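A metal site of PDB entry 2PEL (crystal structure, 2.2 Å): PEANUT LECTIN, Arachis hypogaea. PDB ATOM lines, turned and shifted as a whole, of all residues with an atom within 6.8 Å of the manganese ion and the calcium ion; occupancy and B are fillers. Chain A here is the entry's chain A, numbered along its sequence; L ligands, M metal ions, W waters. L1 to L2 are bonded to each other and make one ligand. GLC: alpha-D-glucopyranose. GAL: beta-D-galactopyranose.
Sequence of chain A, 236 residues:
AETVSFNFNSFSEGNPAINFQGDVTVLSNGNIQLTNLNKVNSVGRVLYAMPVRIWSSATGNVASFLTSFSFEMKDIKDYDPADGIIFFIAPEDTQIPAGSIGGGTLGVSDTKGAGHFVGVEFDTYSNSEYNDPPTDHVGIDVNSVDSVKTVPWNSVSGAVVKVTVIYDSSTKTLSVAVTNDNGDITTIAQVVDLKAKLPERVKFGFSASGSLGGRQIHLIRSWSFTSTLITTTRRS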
ATOM      1  N   ASP A  83     -13.280  22.323   7.114  1.00  0.00           N
ATOM      2  CA  ASP A  83     -12.782  22.267   8.483  1.00  0.00           C
ATOM      3  C   ASP A  83     -13.512  23.178   9.467  1.00  0.00           C
ATOM      4  O   ASP A  83     -13.330  22.970  10.675  1.00  0.00           O
ATOM      5  CB  ASP A  83     -11.285  22.641   8.361  1.00  0.00           C
ATOM      6  CG  ASP A  83     -10.422  21.406   8.158  1.00  0.00           C
ATOM      7  OD1 ASP A  83      -9.987  20.749   9.128  1.00  0.00           O
ATOM      8  OD2 ASP A  83     -10.183  21.093   6.971  1.00  0.00           O
ATOM      9  N   GLY A 103      -6.767  23.424   5.923  1.00  0.00           N
ATOM     10  CA  GLY A 103      -7.124  22.452   6.937  1.00  0.00           C
ATOM     11  C   GLY A 103      -7.480  23.062   8.291  1.00  0.00           C
ATOM     12  O   GLY A 103      -8.207  24.046   8.414  1.00  0.00           O
ATOM     13  N   GLY A 104      -6.920  22.411   9.321  1.00  0.00           N
ATOM     14  CA  GLY A 104      -7.105  22.718  10.729  1.00  0.00           C
ATOM     15  C   GLY A 104      -6.512  24.009  11.247  1.00  0.00           C
ATOM     16  O   GLY A 104      -6.629  24.284  12.466  1.00  0.00           O
ATOM     17  N   THR A 105      -5.883  24.753  10.357  1.00  0.00           N
ATOM     18  CA  THR A 105      -5.257  26.038  10.709  1.00  0.00           C
ATOM     19  C   THR A 105      -6.328  27.121  10.552  1.00  0.00           C
ATOM     20  O   THR A 105      -6.108  28.256  11.000  1.00  0.00           O
ATOM     21  CB  THR A 105      -3.995  26.415   9.849  1.00  0.00           C
ATOM     22  OG1 THR A 105      -4.520  26.596   8.490  1.00  0.00           O
ATOM     23  CG2 THR A 105      -2.812  25.460   9.776  1.00  0.00           C
ATOM     24  N   LEU A 106      -7.416  26.762   9.902  1.00  0.00           N
ATOM     25  CA  LEU A 106      -8.584  27.593   9.625  1.00  0.00           C
ATOM     26  C   LEU A 106      -8.304  28.887   8.860  1.00  0.00           C
ATOM     27  O   LEU A 106      -9.064  29.882   8.918  1.00  0.00           O
ATOM     28  CB  LEU A 106      -9.323  27.825  10.974  1.00  0.00           C
ATOM     29  CG  LEU A 106      -9.825  26.588  11.722  1.00  0.00           C
ATOM     30  CD1 LEU A 106     -10.452  26.930  13.073  1.00  0.00           C
ATOM     31  CD2 LEU A 106     -10.883  25.859  10.875  1.00  0.00           C
ATOM     32  N   GLU A 121     -14.020  29.859  17.091  1.00  0.00           N
ATOM     33  CA  GLU A 121     -14.095  28.850  15.997  1.00  0.00           C
ATOM     34  C   GLU A 121     -15.268  27.874  16.092  1.00  0.00           C
ATOM     35  O   GLU A 121     -15.765  27.515  17.171  1.00  0.00           O
ATOM     36  CB  GLU A 121     -12.822  28.011  16.000  1.00  0.00           C
ATOM     37  CG  GLU A 121     -12.475  27.301  17.298  1.00  0.00           C
ATOM     38  CD  GLU A 121     -11.360  26.309  17.120  1.00  0.00           C
ATOM     39  OE1 GLU A 121     -10.213  26.722  17.077  1.00  0.00           O
ATOM     40  OE2 GLU A 121     -11.726  25.129  16.987  1.00  0.00           O
ATOM     41  N   ASP A 123     -15.481  24.620  14.888  1.00  0.00           N
ATOM     42  CA  ASP A 123     -14.614  23.558  14.318  1.00  0.00           C
ATOM     43  C   ASP A 123     -15.295  22.226  14.058  1.00  0.00           C
ATOM     44  O   ASP A 123     -15.694  21.584  15.033  1.00  0.00           O
ATOM     45  CB  ASP A 123     -13.398  23.500  15.230  1.00  0.00           C
ATOM     46  CG  ASP A 123     -12.231  22.736  14.675  1.00  0.00           C
ATOM     47  OD1 ASP A 123     -12.363  21.915  13.734  1.00  0.00           O
ATOM     48  OD2 ASP A 123     -11.113  22.947  15.188  1.00  0.00           O
ATOM     49  N   THR A 124     -15.354  21.834  12.779  1.00  0.00           N
ATOM     50  CA  THR A 124     -16.003  20.568  12.415  1.00  0.00           C
ATOM     51  C   THR A 124     -15.098  19.385  12.137  1.00  0.00           C
ATOM     52  O   THR A 124     -15.606  18.378  11.583  1.00  0.00           O
ATOM     53  CB  THR A 124     -16.958  20.717  11.168  1.00  0.00           C
ATOM     54  OG1 THR A 124     -16.087  20.784   9.997  1.00  0.00           O
ATOM     55  CG2 THR A 124     -17.913  21.900  11.267  1.00  0.00           C
ATOM     56  N   TYR A 125     -13.831  19.452  12.459  1.00  0.00           N
ATOM     57  CA  TYR A 125     -12.933  18.304  12.174  1.00  0.00           C
ATOM     58  C   TYR A 125     -11.933  18.228  13.317  1.00  0.00           C
ATOM     59  O   TYR A 125     -11.362  19.274  13.665  1.00  0.00           O
ATOM     60  CB  TYR A 125     -12.209  18.410  10.808  1.00  0.00           C
ATOM     61  CG  TYR A 125     -11.296  17.201  10.663  1.00  0.00           C
ATOM     62  CD1 TYR A 125      -9.975  17.261  11.154  1.00  0.00           C
ATOM     63  CD2 TYR A 125     -11.771  16.013  10.100  1.00  0.00           C
ATOM     64  CE1 TYR A 125      -9.155  16.144  11.080  1.00  0.00           C
ATOM     65  CE2 TYR A 125     -10.946  14.889  10.015  1.00  0.00           C
ATOM     66  CZ  TYR A 125      -9.638  14.968  10.488  1.00  0.00           C
ATOM     67  OH  TYR A 125      -8.793  13.889  10.421  1.00  0.00           O
ATOM     68  N   SER A 126     -11.659  17.039  13.804  1.00  0.00           N
ATOM     69  CA  SER A 126     -10.718  16.901  14.924  1.00  0.00           C
ATOM     70  C   SER A 126      -9.269  16.663  14.566  1.00  0.00           C
ATOM     71  O   SER A 126      -8.904  15.534  14.177  1.00  0.00           O
ATOM     72  CB  SER A 126     -11.296  15.793  15.807  1.00  0.00           C
ATOM     73  OG  SER A 126     -10.590  15.726  17.037  1.00  0.00           O
ATOM     74  N   ASN A 127      -8.459  17.693  14.746  1.00  0.00           N
ATOM     75  CA  ASN A 127      -7.023  17.704  14.471  1.00  0.00           C
ATOM     76  C   ASN A 127      -6.287  17.471  15.795  1.00  0.00           C
ATOM     77  O   ASN A 127      -6.224  18.404  16.612  1.00  0.00           O
ATOM     78  CB  ASN A 127      -6.506  19.016  13.862  1.00  0.00           C
ATOM     79  CG  ASN A 127      -7.233  19.356  12.583  1.00  0.00           C
ATOM     80  OD1 ASN A 127      -8.290  20.011  12.679  1.00  0.00           O
ATOM     81  ND2 ASN A 127      -6.754  18.974  11.402  1.00  0.00           N
ATOM     82  N   TYR A 130      -3.484  19.816  16.900  1.00  0.00           N
ATOM     83  CA  TYR A 130      -3.826  21.079  17.588  1.00  0.00           C
ATOM     84  C   TYR A 130      -4.695  20.751  18.803  1.00  0.00           C
ATOM     85  O   TYR A 130      -5.466  21.621  19.221  1.00  0.00           O
ATOM     86  CB  TYR A 130      -4.556  22.063  16.672  1.00  0.00           C
ATOM     87  CG  TYR A 130      -3.842  22.220  15.351  1.00  0.00           C
ATOM     88  CD1 TYR A 130      -2.515  22.635  15.324  1.00  0.00           C
ATOM     89  CD2 TYR A 130      -4.478  21.931  14.145  1.00  0.00           C
ATOM     90  CE1 TYR A 130      -1.840  22.796  14.107  1.00  0.00           C
ATOM     91  CE2 TYR A 130      -3.836  22.089  12.933  1.00  0.00           C
ATOM     92  CZ  TYR A 130      -2.515  22.525  12.917  1.00  0.00           C
ATOM     93  OH  TYR A 130      -1.843  22.665  11.746  1.00  0.00           O
ATOM     94  N   ASN A 131      -4.547  19.556  19.299  1.00  0.00           N
ATOM     95  CA  ASN A 131      -5.248  19.030  20.467  1.00  0.00           C
ATOM     96  C   ASN A 131      -6.762  19.257  20.443  1.00  0.00           C
ATOM     97  O   ASN A 131      -7.304  19.681  21.483  1.00  0.00           O
ATOM     98  CB  ASN A 131      -4.678  19.605  21.773  1.00  0.00           C
ATOM     99  CG  ASN A 131      -3.205  19.299  21.942  1.00  0.00           C
ATOM    100  OD1 ASN A 131      -2.748  18.173  21.653  1.00  0.00           O
ATOM    101  ND2 ASN A 131      -2.461  20.306  22.432  1.00  0.00           N
ATOM    102  N   ASP A 132      -7.402  18.983  19.323  1.00  0.00           N
ATOM    103  CA  ASP A 132      -8.842  19.180  19.243  1.00  0.00           C
ATOM    104  C   ASP A 132      -9.625  18.166  20.068  1.00  0.00           C
ATOM    105  O   ASP A 132      -9.198  17.014  20.143  1.00  0.00           O
ATOM    106  CB  ASP A 132      -9.254  18.959  17.786  1.00  0.00           C
ATOM    107  CG  ASP A 132      -9.285  20.252  16.974  1.00  0.00           C
ATOM    108  OD1 ASP A 132      -9.177  21.321  17.588  1.00  0.00           O
ATOM    109  OD2 ASP A 132      -9.399  19.998  15.756  1.00  0.00           O
ATOM    110  N   PRO A 133     -10.769  18.605  20.598  1.00  0.00           N
ATOM    111  CA  PRO A 133     -11.662  17.700  21.328  1.00  0.00           C
ATOM    112  C   PRO A 133     -12.110  16.691  20.238  1.00  0.00           C
ATOM    113  O   PRO A 133     -12.034  16.938  19.007  1.00  0.00           O
ATOM    114  CB  PRO A 133     -12.778  18.589  21.830  1.00  0.00           C
ATOM    115  CG  PRO A 133     -12.196  19.992  21.775  1.00  0.00           C
ATOM    116  CD  PRO A 133     -11.333  19.950  20.524  1.00  0.00           C
ATOM    117  N   HIS A 137     -17.053  21.280  17.796  1.00  0.00           N
ATOM    118  CA  HIS A 137     -16.961  22.177  18.954  1.00  0.00           C
ATOM    119  C   HIS A 137     -16.782  23.653  18.653  1.00  0.00           C
ATOM    120  O   HIS A 137     -16.413  24.000  17.525  1.00  0.00           O
ATOM    121  CB  HIS A 137     -15.765  21.734  19.858  1.00  0.00           C
ATOM    122  CG  HIS A 137     -14.476  21.681  19.090  1.00  0.00           C
ATOM    123  ND1 HIS A 137     -14.151  20.642  18.225  1.00  0.00           N
ATOM    124  CD2 HIS A 137     -13.432  22.568  19.080  1.00  0.00           C
ATOM    125  CE1 HIS A 137     -12.955  20.897  17.735  1.00  0.00           C
ATOM    126  NE2 HIS A 137     -12.502  22.033  18.223  1.00  0.00           N
ATOM    127  N   VAL A 138     -17.033  24.425  19.701  1.00  0.00           N
ATOM    128  CA  VAL A 138     -16.870  25.918  19.700  1.00  0.00           C
ATOM    129  C   VAL A 138     -15.657  26.122  20.619  1.00  0.00           C
ATOM    130  O   VAL A 138     -15.505  25.447  21.653  1.00  0.00           O
ATOM    131  CB  VAL A 138     -18.147  26.620  20.137  1.00  0.00           C
ATOM    132  CG1 VAL A 138     -18.082  28.131  20.029  1.00  0.00           C
ATOM    133  CG2 VAL A 138     -19.396  26.109  19.411  1.00  0.00           C
ATOM    134  N   GLY A 139     -14.708  26.966  20.250  1.00  0.00           N
ATOM    135  CA  GLY A 139     -13.502  27.169  21.088  1.00  0.00           C
ATOM    136  C   GLY A 139     -13.169  28.656  21.016  1.00  0.00           C
ATOM    137  O   GLY A 139     -13.624  29.375  20.114  1.00  0.00           O
ATOM    138  N   ASP A 141      -9.976  31.027  20.806  1.00  0.00           N
ATOM    139  CA  ASP A 141      -8.563  30.914  20.428  1.00  0.00           C
ATOM    140  C   ASP A 141      -7.774  32.192  20.697  1.00  0.00           C
ATOM    141  O   ASP A 141      -8.266  33.211  20.207  1.00  0.00           O
ATOM    142  CB  ASP A 141      -8.502  30.601  18.926  1.00  0.00           C
ATOM    143  CG  ASP A 141      -9.105  29.261  18.546  1.00  0.00           C
ATOM    144  OD1 ASP A 141      -9.661  28.560  19.425  1.00  0.00           O
ATOM    145  OD2 ASP A 141      -9.070  28.844  17.385  1.00  0.00           O
ATOM    146  N   VAL A 145      -4.593  27.793  17.299  1.00  0.00           N
ATOM    147  CA  VAL A 145      -5.810  27.008  17.033  1.00  0.00           C
ATOM    148  C   VAL A 145      -5.902  25.884  18.095  1.00  0.00           C
ATOM    149  O   VAL A 145      -6.746  24.973  18.040  1.00  0.00           O
ATOM    150  CB  VAL A 145      -5.974  26.462  15.615  1.00  0.00           C
ATOM    151  CG1 VAL A 145      -6.530  27.519  14.661  1.00  0.00           C
ATOM    152  CG2 VAL A 145      -4.698  25.773  15.160  1.00  0.00           C
ATOM    153  N   ASP A 146      -5.008  25.974  19.066  1.00  0.00           N
ATOM    154  CA  ASP A 146      -4.969  25.041  20.221  1.00  0.00           C
ATOM    155  C   ASP A 146      -5.712  25.944  21.257  1.00  0.00           C
ATOM    156  O   ASP A 146      -5.099  26.764  21.978  1.00  0.00           O
ATOM    157  CB  ASP A 146      -3.611  24.549  20.626  1.00  0.00           C
ATOM    158  CG  ASP A 146      -3.594  23.586  21.798  1.00  0.00           C
ATOM    159  OD1 ASP A 146      -4.674  23.300  22.367  1.00  0.00           O
ATOM    160  OD2 ASP A 146      -2.514  23.096  22.186  1.00  0.00           O
ATOM    161  N   SER A 147      -7.016  25.778  21.190  1.00  0.00           N
ATOM    162  CA  SER A 147      -7.963  26.545  22.015  1.00  0.00           C
ATOM    163  C   SER A 147      -7.673  26.485  23.524  1.00  0.00           C
ATOM    164  O   SER A 147      -7.368  25.493  24.188  1.00  0.00           O
ATOM    165  CB  SER A 147      -9.409  26.192  21.768  1.00  0.00           C
ATOM    166  OG  SER A 147      -9.836  26.284  20.434  1.00  0.00           O
ATOM    167  N   THR A 150     -12.719  25.023  25.080  1.00  0.00           N
ATOM    168  CA  THR A 150     -13.694  24.535  24.100  1.00  0.00           C
ATOM    169  C   THR A 150     -14.930  23.952  24.795  1.00  0.00           C
ATOM    170  O   THR A 150     -14.918  23.606  25.966  1.00  0.00           O
ATOM    171  CB  THR A 150     -13.081  23.422  23.150  1.00  0.00           C
ATOM    172  OG1 THR A 150     -12.977  22.279  24.072  1.00  0.00           O
ATOM    173  CG2 THR A 150     -11.765  23.792  22.476  1.00  0.00           C
HETATM  174  C1  GLC L   1      -4.213  13.287   3.258  1.00  0.00           C
HETATM  175  C2  GLC L   1      -5.654  13.673   2.967  1.00  0.00           C
HETATM  176  C3  GLC L   1      -5.886  15.101   3.501  1.00  0.00           C
HETATM  177  C4  GLC L   1      -5.637  15.073   5.025  1.00  0.00           C
HETATM  178  C5  GLC L   1      -4.223  14.592   5.316  1.00  0.00           C
HETATM  179  C6  GLC L   1      -3.876  14.367   6.764  1.00  0.00           C
HETATM  180  O1  GLC L   1      -3.470  14.320   2.518  1.00  0.00           O
HETATM  181  O2  GLC L   1      -5.854  13.507   1.509  1.00  0.00           O
HETATM  182  O3  GLC L   1      -7.271  15.403   3.444  1.00  0.00           O
HETATM  183  O4  GLC L   1      -6.021  16.337   5.563  1.00  0.00           O
HETATM  184  O5  GLC L   1      -3.986  13.355   4.637  1.00  0.00           O
HETATM  185  O6  GLC L   1      -4.772  13.418   7.414  1.00  0.00           O
HETATM  186  C1  GAL L   2      -6.863  16.401   6.687  1.00  0.00           C
HETATM  187  C2  GAL L   2      -6.709  17.822   7.235  1.00  0.00           C
HETATM  188  C3  GAL L   2      -7.812  18.171   8.188  1.00  0.00           C
HETATM  189  C4  GAL L   2      -9.174  17.914   7.578  1.00  0.00           C
HETATM  190  C5  GAL L   2      -9.216  16.442   7.189  1.00  0.00           C
HETATM  191  C6  GAL L   2     -10.492  16.029   6.524  1.00  0.00           C
HETATM  192  O2  GAL L   2      -5.440  18.026   7.774  1.00  0.00           O
HETATM  193  O3  GAL L   2      -7.661  19.485   8.737  1.00  0.00           O
HETATM  194  O4  GAL L   2      -9.518  18.654   6.395  1.00  0.00           O
HETATM  195  O5  GAL L   2      -8.173  16.179   6.210  1.00  0.00           O
HETATM  196  O6  GAL L   2     -10.327  14.682   6.116  1.00  0.00           O
HETATM  197 MN    MN M   1     -10.585  23.147  17.421  1.00  0.00          MN
HETATM  198 CA    CA M   2     -10.005  21.243  13.805  1.00  0.00          CA
HETATM  199  O   HOH W   1      -8.427  23.044  14.195  1.00  0.00           O
HETATM  200  O   HOH W   2      -9.832  23.779  19.539  1.00  0.00           O
HETATM  201  O   HOH W   3     -10.769  21.838  11.593  1.00  0.00           O
HETATM  202  O   HOH W   4      -8.866  24.326  16.441  1.00  0.00           O
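The side-chain carboxylate (OD2) of Asp 83 lies within hydrogen-bond range of an oxygen (O4) of GAL L2 (2.6 Å). The side-chain amide nitrogen (ND2) of Asn 127 sits at hydrogen-bond distance from an oxygen (O3) of GAL L2, 2.9 Å away. An oxygen (O3) of GAL L2 lies within hydrogen-bond range of the backbone NH (N) of Gly 104 (3.1 Å).
The side-chain carboxylate (OE1) of Glu 121 lies within hydrogen-bond range of the side-chain hydroxyl (OG) of Ser 147, 3.4 Å away. The backbone NH (N) of Glu 121 lies within hydrogen-bond range of the backbone carbonyl oxygen (O) of Gly 139 (3.1 Å). The side-chain carboxylate (OE1) of Glu 121 lies close to the side-chain carboxylate (OD2) of Asp 141 (2.4 Å).
The nearest printed residue that does not touch the manganese ion is Val 145 (4.3 Å).
The nearest printed residue that does not touch the calcium ion is Gly 104 (4.5 Å).
The manganese ion is bound by water W4 (2.3 Å), OD2 of Asp 123 (2.3 Å), OD1 of Asp 132 (2.3 Å), OE2 of Glu 121 (2.3 Å), water W2 (2.3 Å) and NE2 of His 137 (2.4 Å).
The calcium ion is bound by OD2 of Asp 132 (2.4 Å), OD1 of Asn 127 (2.4 Å), O of Tyr 125 (2.4 Å), water W3 (2.4 Å), water W1 (2.4 Å), OD1 of Asp 123 (2.5 Å) and OD2 of Asp 123 (2.5 Å). The calcium ion has seven donor atoms within binding distance.
Water W4 lies within hydrogen-bond range of O of Val 145 and OE1 of Glu 121.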
